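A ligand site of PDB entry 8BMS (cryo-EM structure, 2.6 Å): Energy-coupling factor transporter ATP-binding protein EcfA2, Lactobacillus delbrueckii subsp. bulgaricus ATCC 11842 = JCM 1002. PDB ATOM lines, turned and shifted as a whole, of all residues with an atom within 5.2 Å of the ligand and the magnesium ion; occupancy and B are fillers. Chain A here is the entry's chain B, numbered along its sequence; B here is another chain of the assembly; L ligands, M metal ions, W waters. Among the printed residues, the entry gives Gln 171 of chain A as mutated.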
ATOM      1  N   TYR A  12     -29.165 -16.733  37.374  1.00  0.00           N
ATOM      2  CA  TYR A  12     -27.880 -16.190  37.818  1.00  0.00           C
ATOM      3  C   TYR A  12     -28.131 -15.071  38.823  1.00  0.00           C
ATOM      4  O   TYR A  12     -28.794 -14.083  38.498  1.00  0.00           O
ATOM      5  CB  TYR A  12     -27.076 -15.676  36.638  1.00  0.00           C
ATOM      6  CG  TYR A  12     -26.405 -16.750  35.805  1.00  0.00           C
ATOM      7  CD1 TYR A  12     -25.225 -17.345  36.232  1.00  0.00           C
ATOM      8  CD2 TYR A  12     -26.944 -17.164  34.601  1.00  0.00           C
ATOM      9  CE1 TYR A  12     -24.602 -18.318  35.481  1.00  0.00           C
ATOM     10  CE2 TYR A  12     -26.330 -18.139  33.839  1.00  0.00           C
ATOM     11  CZ  TYR A  12     -25.160 -18.712  34.288  1.00  0.00           C
ATOM     12  OH  TYR A  12     -24.546 -19.683  33.536  1.00  0.00           O
ATOM     13  N   ALA A  20     -30.759 -12.567  36.324  1.00  0.00           N
ATOM     14  CA  ALA A  20     -30.885 -13.017  34.943  1.00  0.00           C
ATOM     15  C   ALA A  20     -31.232 -14.506  34.940  1.00  0.00           C
ATOM     16  O   ALA A  20     -30.599 -15.288  35.654  1.00  0.00           O
ATOM     17  CB  ALA A  20     -29.602 -12.767  34.154  1.00  0.00           C
ATOM     18  N   GLY A  22     -30.845 -17.750  33.425  1.00  0.00           N
ATOM     19  CA  GLY A  22     -30.007 -18.466  32.480  1.00  0.00           C
ATOM     20  C   GLY A  22     -30.768 -19.523  31.708  1.00  0.00           C
ATOM     21  O   GLY A  22     -30.622 -19.643  30.489  1.00  0.00           O
ATOM     22  N   HIS A  41     -28.178 -19.147  19.759  1.00  0.00           N
ATOM     23  CA  HIS A  41     -27.450 -17.893  19.648  1.00  0.00           C
ATOM     24  C   HIS A  41     -26.538 -17.706  20.855  1.00  0.00           C
ATOM     25  O   HIS A  41     -26.587 -18.458  21.824  1.00  0.00           O
ATOM     26  CB  HIS A  41     -28.423 -16.718  19.518  1.00  0.00           C
ATOM     27  CG  HIS A  41     -29.299 -16.511  20.710  1.00  0.00           C
ATOM     28  ND1 HIS A  41     -28.953 -15.668  21.749  1.00  0.00           N
ATOM     29  CD2 HIS A  41     -30.507 -17.023  21.029  1.00  0.00           C
ATOM     30  CE1 HIS A  41     -29.911 -15.684  22.659  1.00  0.00           C
ATOM     31  NE2 HIS A  41     -30.866 -16.500  22.246  1.00  0.00           N
ATOM     32  N   THR A  42     -25.679 -16.687  20.784  1.00  0.00           N
ATOM     33  CA  THR A  42     -24.806 -16.384  21.903  1.00  0.00           C
ATOM     34  C   THR A  42     -25.618 -15.905  23.089  1.00  0.00           C
ATOM     35  O   THR A  42     -26.522 -15.080  22.957  1.00  0.00           O
ATOM     36  CB  THR A  42     -23.776 -15.320  21.508  1.00  0.00           C
ATOM     37  OG1 THR A  42     -24.444 -14.169  20.988  1.00  0.00           O
ATOM     38  CG2 THR A  42     -22.821 -15.864  20.452  1.00  0.00           C
ATOM     39  N   GLY A  43     -25.297 -16.440  24.269  1.00  0.00           N
ATOM     40  CA  GLY A  43     -26.039 -16.095  25.466  1.00  0.00           C
ATOM     41  C   GLY A  43     -27.384 -16.756  25.597  1.00  0.00           C
ATOM     42  O   GLY A  43     -28.241 -16.250  26.327  1.00  0.00           O
ATOM     43  N   SER A  44     -27.621 -17.868  24.897  1.00  0.00           N
ATOM     44  CA  SER A  44     -28.898 -18.566  24.952  1.00  0.00           C
ATOM     45  C   SER A  44     -28.982 -19.594  26.063  1.00  0.00           C
ATOM     46  O   SER A  44     -30.060 -20.152  26.293  1.00  0.00           O
ATOM     47  CB  SER A  44     -29.190 -19.239  23.611  1.00  0.00           C
ATOM     48  OG  SER A  44     -28.169 -20.142  23.260  1.00  0.00           O
ATOM     49  N   GLY A  45     -27.888 -19.881  26.752  1.00  0.00           N
ATOM     50  CA  GLY A  45     -27.873 -20.814  27.852  1.00  0.00           C
ATOM     51  C   GLY A  45     -27.254 -22.170  27.579  1.00  0.00           C
ATOM     52  O   GLY A  45     -27.579 -23.127  28.286  1.00  0.00           O
ATOM     53  N   LYS A  46     -26.365 -22.283  26.589  1.00  0.00           N
ATOM     54  CA  LYS A  46     -25.746 -23.559  26.270  1.00  0.00           C
ATOM     55  C   LYS A  46     -24.680 -23.953  27.289  1.00  0.00           C
ATOM     56  O   LYS A  46     -24.622 -25.107  27.712  1.00  0.00           O
ATOM     57  CB  LYS A  46     -25.153 -23.506  24.859  1.00  0.00           C
ATOM     58  CG  LYS A  46     -26.159 -23.100  23.796  1.00  0.00           C
ATOM     59  CD  LYS A  46     -25.604 -23.228  22.386  1.00  0.00           C
ATOM     60  CE  LYS A  46     -24.395 -22.333  22.182  1.00  0.00           C
ATOM     61  NZ  LYS A  46     -24.756 -20.900  22.070  1.00  0.00           N
ATOM     62  N   SER A  47     -23.848 -22.997  27.705  1.00  0.00           N
ATOM     63  CA  SER A  47     -22.824 -23.293  28.699  1.00  0.00           C
ATOM     64  C   SER A  47     -23.435 -23.571  30.066  1.00  0.00           C
ATOM     65  O   SER A  47     -22.918 -24.415  30.808  1.00  0.00           O
ATOM     66  CB  SER A  47     -21.825 -22.141  28.779  1.00  0.00           C
ATOM     67  OG  SER A  47     -21.330 -21.797  27.505  1.00  0.00           O
ATOM     68  N   THR A  48     -24.527 -22.883  30.396  1.00  0.00           N
ATOM     69  CA  THR A  48     -25.235 -23.197  31.627  1.00  0.00           C
ATOM     70  C   THR A  48     -25.793 -24.616  31.597  1.00  0.00           C
ATOM     71  O   THR A  48     -25.727 -25.341  32.586  1.00  0.00           O
ATOM     72  CB  THR A  48     -26.361 -22.180  31.852  1.00  0.00           C
ATOM     73  OG1 THR A  48     -25.822 -20.859  31.771  1.00  0.00           O
ATOM     74  CG2 THR A  48     -26.979 -22.366  33.221  1.00  0.00           C
ATOM     75  N   GLN A  92     -15.716 -24.075  27.642  1.00  0.00           N
ATOM     76  CA  GLN A  92     -15.606 -23.197  26.479  1.00  0.00           C
ATOM     77  C   GLN A  92     -14.223 -22.567  26.398  1.00  0.00           C
ATOM     78  O   GLN A  92     -13.649 -22.437  25.314  1.00  0.00           O
ATOM     79  CB  GLN A  92     -16.685 -22.117  26.536  1.00  0.00           C
ATOM     80  CG  GLN A  92     -16.613 -21.097  25.427  1.00  0.00           C
ATOM     81  CD  GLN A  92     -17.950 -20.455  25.130  1.00  0.00           C
ATOM     82  OE1 GLN A  92     -18.828 -20.399  25.993  1.00  0.00           O
ATOM     83  NE2 GLN A  92     -18.106 -19.951  23.912  1.00  0.00           N
ATOM     84  N   ASP A 170     -18.030 -27.908  25.137  1.00  0.00           N
ATOM     85  CA  ASP A 170     -18.467 -26.531  24.932  1.00  0.00           C
ATOM     86  C   ASP A 170     -17.591 -25.895  23.869  1.00  0.00           C
ATOM     87  O   ASP A 170     -16.543 -25.316  24.166  1.00  0.00           O
ATOM     88  CB  ASP A 170     -18.415 -25.767  26.255  1.00  0.00           C
ATOM     89  CG  ASP A 170     -19.481 -24.696  26.351  1.00  0.00           C
ATOM     90  OD1 ASP A 170     -20.082 -24.360  25.312  1.00  0.00           O
ATOM     91  OD2 ASP A 170     -19.715 -24.199  27.470  1.00  0.00           O
ATOM     92  N   GLN A 171     -18.023 -25.996  22.623  1.00  0.00           N
ATOM     93  CA  GLN A 171     -17.303 -25.463  21.470  1.00  0.00           C
ATOM     94  C   GLN A 171     -15.855 -25.941  21.430  1.00  0.00           C
ATOM     95  O   GLN A 171     -14.925 -25.134  21.471  1.00  0.00           O
ATOM     96  CB  GLN A 171     -17.369 -23.944  21.456  1.00  0.00           C
ATOM     97  CG  GLN A 171     -18.749 -23.389  21.216  1.00  0.00           C
ATOM     98  CD  GLN A 171     -18.736 -21.910  20.863  1.00  0.00           C
ATOM     99  OE1 GLN A 171     -17.986 -21.489  19.984  1.00  0.00           O
ATOM    100  NE2 GLN A 171     -19.563 -21.134  21.541  1.00  0.00           N
ATOM    101  N   HIS A 203     -21.292 -23.719  16.991  1.00  0.00           N
ATOM    102  CA  HIS A 203     -21.833 -22.624  16.200  1.00  0.00           C
ATOM    103  C   HIS A 203     -21.704 -22.869  14.706  1.00  0.00           C
ATOM    104  O   HIS A 203     -21.956 -21.966  13.905  1.00  0.00           O
ATOM    105  CB  HIS A 203     -21.153 -21.304  16.583  1.00  0.00           C
ATOM    106  CG  HIS A 203     -21.685 -20.684  17.830  1.00  0.00           C
ATOM    107  ND1 HIS A 203     -23.034 -20.541  18.074  1.00  0.00           N
ATOM    108  CD2 HIS A 203     -21.059 -20.166  18.907  1.00  0.00           C
ATOM    109  CE1 HIS A 203     -23.214 -19.965  19.251  1.00  0.00           C
ATOM    110  NE2 HIS A 203     -22.029 -19.720  19.775  1.00  0.00           N
ATOM    111  N   TYR B 136     -26.806  -5.110  27.375  1.00  0.00           N
ATOM    112  CA  TYR B 136     -25.808  -5.515  28.360  1.00  0.00           C
ATOM    113  C   TYR B 136     -24.820  -4.394  28.673  1.00  0.00           C
ATOM    114  O   TYR B 136     -23.739  -4.669  29.200  1.00  0.00           O
ATOM    115  CB  TYR B 136     -25.056  -6.755  27.883  1.00  0.00           C
ATOM    116  CG  TYR B 136     -25.897  -8.008  27.807  1.00  0.00           C
ATOM    117  CD1 TYR B 136     -26.019  -8.851  28.888  1.00  0.00           C
ATOM    118  CD2 TYR B 136     -26.560  -8.338  26.631  1.00  0.00           C
ATOM    119  CE1 TYR B 136     -26.793  -9.992  28.823  1.00  0.00           C
ATOM    120  CE2 TYR B 136     -27.334  -9.482  26.558  1.00  0.00           C
ATOM    121  CZ  TYR B 136     -27.443 -10.302  27.651  1.00  0.00           C
ATOM    122  OH  TYR B 136     -28.217 -11.446  27.577  1.00  0.00           O
ATOM    123  N   SER B 142     -17.074  -9.743  32.760  1.00  0.00           N
ATOM    124  CA  SER B 142     -16.759 -11.106  33.167  1.00  0.00           C
ATOM    125  C   SER B 142     -18.001 -11.967  33.353  1.00  0.00           C
ATOM    126  O   SER B 142     -17.904 -13.190  33.272  1.00  0.00           O
ATOM    127  CB  SER B 142     -15.939 -11.096  34.457  1.00  0.00           C
ATOM    128  OG  SER B 142     -16.745 -10.781  35.573  1.00  0.00           O
ATOM    129  N   ASN B 143     -19.155 -11.352  33.612  1.00  0.00           N
ATOM    130  CA  ASN B 143     -20.417 -12.079  33.736  1.00  0.00           C
ATOM    131  C   ASN B 143     -21.137 -12.155  32.398  1.00  0.00           C
ATOM    132  O   ASN B 143     -22.313 -11.810  32.270  1.00  0.00           O
ATOM    133  CB  ASN B 143     -21.300 -11.409  34.786  1.00  0.00           C
ATOM    134  CG  ASN B 143     -20.765 -11.596  36.193  1.00  0.00           C
ATOM    135  OD1 ASN B 143     -19.940 -12.472  36.450  1.00  0.00           O
ATOM    136  ND2 ASN B 143     -21.232 -10.766  37.109  1.00  0.00           N
ATOM    137  N   LEU B 144     -20.429 -12.610  31.368  1.00  0.00           N
ATOM    138  CA  LEU B 144     -20.955 -12.701  30.020  1.00  0.00           C
ATOM    139  C   LEU B 144     -20.582 -14.059  29.430  1.00  0.00           C
ATOM    140  O   LEU B 144     -19.682 -14.743  29.916  1.00  0.00           O
ATOM    141  CB  LEU B 144     -20.409 -11.591  29.111  1.00  0.00           C
ATOM    142  CG  LEU B 144     -20.761 -10.136  29.418  1.00  0.00           C
ATOM    143  CD1 LEU B 144     -20.049  -9.218  28.434  1.00  0.00           C
ATOM    144  CD2 LEU B 144     -22.255  -9.908  29.369  1.00  0.00           C
ATOM    145  N   SER B 145     -21.318 -14.446  28.394  1.00  0.00           N
ATOM    146  CA  SER B 145     -20.955 -15.638  27.641  1.00  0.00           C
ATOM    147  C   SER B 145     -19.747 -15.362  26.768  1.00  0.00           C
ATOM    148  O   SER B 145     -19.289 -14.225  26.631  1.00  0.00           O
ATOM    149  CB  SER B 145     -22.146 -16.115  26.802  1.00  0.00           C
ATOM    150  OG  SER B 145     -22.369 -15.269  25.700  1.00  0.00           O
ATOM    151  N   GLY B 146     -19.204 -16.428  26.173  1.00  0.00           N
ATOM    152  CA  GLY B 146     -18.012 -16.274  25.343  1.00  0.00           C
ATOM    153  C   GLY B 146     -18.242 -15.397  24.127  1.00  0.00           C
ATOM    154  O   GLY B 146     -17.420 -14.529  23.813  1.00  0.00           O
ATOM    155  N   GLY B 147     -19.364 -15.605  23.438  1.00  0.00           N
ATOM    156  CA  GLY B 147     -19.671 -14.761  22.286  1.00  0.00           C
ATOM    157  C   GLY B 147     -19.947 -13.323  22.673  1.00  0.00           C
ATOM    158  O   GLY B 147     -19.563 -12.396  21.952  1.00  0.00           O
ATOM    159  N   GLN B 148     -20.620 -13.119  23.807  1.00  0.00           N
ATOM    160  CA  GLN B 148     -20.862 -11.760  24.288  1.00  0.00           C
ATOM    161  C   GLN B 148     -19.550 -11.070  24.647  1.00  0.00           C
ATOM    162  O   GLN B 148     -19.357  -9.880  24.362  1.00  0.00           O
ATOM    163  CB  GLN B 148     -21.806 -11.792  25.481  1.00  0.00           C
ATOM    164  CG  GLN B 148     -23.228 -12.198  25.129  1.00  0.00           C
ATOM    165  CD  GLN B 148     -24.151 -12.224  26.322  1.00  0.00           C
ATOM    166  OE1 GLN B 148     -23.708 -12.145  27.469  1.00  0.00           O
ATOM    167  NE2 GLN B 148     -25.447 -12.320  26.062  1.00  0.00           N
ATOM    168  N   MET B 173     -16.194 -17.690  18.621  1.00  0.00           N
ATOM    169  CA  MET B 173     -17.271 -18.086  19.515  1.00  0.00           C
ATOM    170  C   MET B 173     -18.574 -17.333  19.237  1.00  0.00           C
ATOM    171  O   MET B 173     -19.410 -17.189  20.120  1.00  0.00           O
ATOM    172  CB  MET B 173     -16.849 -17.893  20.972  1.00  0.00           C
ATOM    173  CG  MET B 173     -15.710 -18.813  21.398  1.00  0.00           C
ATOM    174  SD  MET B 173     -15.187 -18.518  23.093  1.00  0.00           S
ATOM    175  CE  MET B 173     -14.543 -16.860  22.948  1.00  0.00           C
HETATM  176  P1  LIG L   1     -22.030 -18.296  23.864  1.00  0.00           P
HETATM  177  O1  LIG L   1     -21.713 -16.855  23.688  1.00  0.00           O
HETATM  178  O2  LIG L   1     -22.426 -19.002  22.573  1.00  0.00           O
HETATM  179  O3  LIG L   1     -20.922 -19.083  24.557  1.00  0.00           O
HETATM  180  P2  LIG L   1     -23.976 -19.564  25.741  1.00  0.00           P
HETATM  181  O4  LIG L   1     -25.130 -20.204  25.088  1.00  0.00           O
HETATM  182  O5  LIG L   1     -22.866 -20.505  26.206  1.00  0.00           O
HETATM  183  O6  LIG L   1     -23.296 -18.469  24.817  1.00  0.00           O
HETATM  184  P3  LIG L   1     -24.279 -18.791  28.588  1.00  0.00           P
HETATM  185  O7  LIG L   1     -22.869 -18.768  29.023  1.00  0.00           O
HETATM  186  O8  LIG L   1     -25.067 -20.021  29.035  1.00  0.00           O
HETATM  187  O9  LIG L   1     -24.410 -18.693  27.005  1.00  0.00           O
HETATM  188  O10 LIG L   1     -25.050 -17.513  29.091  1.00  0.00           O
HETATM  189  C1  LIG L   1     -26.490 -17.452  29.121  1.00  0.00           C
HETATM  190  C2  LIG L   1     -26.941 -16.120  29.661  1.00  0.00           C
HETATM  191  O11 LIG L   1     -26.503 -15.978  31.033  1.00  0.00           O
HETATM  192  C3  LIG L   1     -26.412 -14.892  28.917  1.00  0.00           C
HETATM  193  O12 LIG L   1     -27.390 -13.857  28.872  1.00  0.00           O
HETATM  194  C4  LIG L   1     -25.189 -14.482  29.745  1.00  0.00           C
HETATM  195  O13 LIG L   1     -24.925 -13.089  29.662  1.00  0.00           O
HETATM  196  C5  LIG L   1     -25.638 -14.854  31.157  1.00  0.00           C
HETATM  197  N1  LIG L   1     -24.547 -15.221  32.046  1.00  0.00           N
HETATM  198  C6  LIG L   1     -23.526 -16.098  31.782  1.00  0.00           C
HETATM  199  N2  LIG L   1     -22.672 -16.246  32.771  1.00  0.00           N
HETATM  200  C7  LIG L   1     -23.169 -15.402  33.756  1.00  0.00           C
HETATM  201  C8  LIG L   1     -22.712 -15.099  35.046  1.00  0.00           C
HETATM  202  N3  LIG L   1     -21.624 -15.630  35.601  1.00  0.00           N
HETATM  203  N4  LIG L   1     -23.437 -14.214  35.772  1.00  0.00           N
HETATM  204  C9  LIG L   1     -24.524 -13.670  35.223  1.00  0.00           C
HETATM  205  N5  LIG L   1     -25.052 -13.891  34.010  1.00  0.00           N
HETATM  206  C10 LIG L   1     -24.320 -14.761  33.322  1.00  0.00           C
HETATM  207 MG    MG M   1     -20.817 -20.292  26.360  1.00  0.00          MG
HETATM  208  O   HOH W   1     -21.766 -19.925  31.684  1.00  0.00           O
HETATM  209  O   HOH W   2     -30.237 -16.610  28.771  1.00  0.00           O
HETATM  210  O   HOH W   3     -24.609 -10.942  31.786  1.00  0.00           O
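The backbone NH (N) of Ser 47 is in hydrogen-bond range of an oxygen (O8) of the ligand (3.5 Å). OG of Ser 145 of chain B is in hydrogen-bond range of O1 of the ligand. An oxygen (O1) of the ligand sits at hydrogen-bond distance from the backbone NH of Gly 147 of chain B (2.7 Å). OE1 of Gln 148 of chain B lies within hydrogen-bond range of O13 of the ligand (2.7 Å). N of Lys 46 lies within hydrogen-bond range of O4 of the ligand (2.8 Å). O2 of the ligand lies within salt-bridge range of NZ of Lys 46, 3.0 Å away. The side-chain hydroxyl (OH) of Tyr 136 of chain B lies within hydrogen-bond range of an oxygen (O12) of the ligand, 2.9 Å away. The backbone NH (N) of Gly 43 lies within hydrogen-bond range of an oxygen (O6) of the ligand (2.9 Å). A ring nitrogen (NE2) of His 203 lies within hydrogen-bond range of an oxygen (O2) of the ligand (2.9 Å). N of Thr 48 sits at hydrogen-bond distance from O8 of the ligand (3.2 Å). OG1 of Thr 48 sits at hydrogen-bond distance from O8 of the ligand. N of Gly 45 sits at hydrogen-bond distance from O4 of the ligand (3.2 Å). An oxygen (O4) of the ligand sits at hydrogen-bond distance from the backbone NH (N) of Ser 44, at 3.4 Å.
OG of Ser 47 sits close to OD2 of Asp 170 (2.9 Å). The side-chain amide nitrogen (NE2) of Gln 92 sits close to the side-chain amide nitrogen (NE2) of Gln 171. OG of Ser 145 of chain B sits close to N of Gln 148 of chain B. N of Gly 43 is in hydrogen-bond range of OG of Ser 145 of chain B (3.5 Å). The side-chain amide nitrogen of Gln 171 sits close to a ring nitrogen (NE2) of His 203 (3.3 Å). The side-chain hydroxyl (OG1) of Thr 48 sits at hydrogen-bond distance from the side-chain hydroxyl (OH) of Tyr 12, 2.5 Å away. O of His 41 sits at hydrogen-bond distance from OG of Ser 44, 2.7 Å away. The backbone NH (N) of Tyr 12 is in hydrogen-bond range of the backbone carbonyl oxygen (O) of Ala 20.
Residues that only touch the ligand: Thr 42, Tyr 12, Gly 146 of chain B, Asn 143 of chain B, Gln 171 and His 41. Hydrophobic or aromatic side chains that line the ligand: Tyr 12, His 203 and Tyr 136 of chain B. The nearest printed residue that does not touch the ligand is Leu 144 of chain B (4.005 Å).
Two residues have an atom within 4 Å of the magnesium ion: Ser 47 and Gln 92. The nearest printed residue that does not touch the magnesium ion is Gly 146 of chain B (4.2 Å).
The magnesium ion is bound by the side-chain hydroxyl (OG) of Ser 47, the side-chain amide oxygen (OE1) of Gln 92, an oxygen (O5) of the ligand and an oxygen (O3) of the ligand. The magnesium ion has four donor atoms within binding distance.
Water W3 bridges the backbone carbonyl oxygen of Asn 143 of chain B (2.5 Å) and an oxygen (O13) of the ligand (3.0 Å). Water W1 bridges O7 of the ligand (3.1 Å) and OH of Tyr 12 (3.3 Å).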
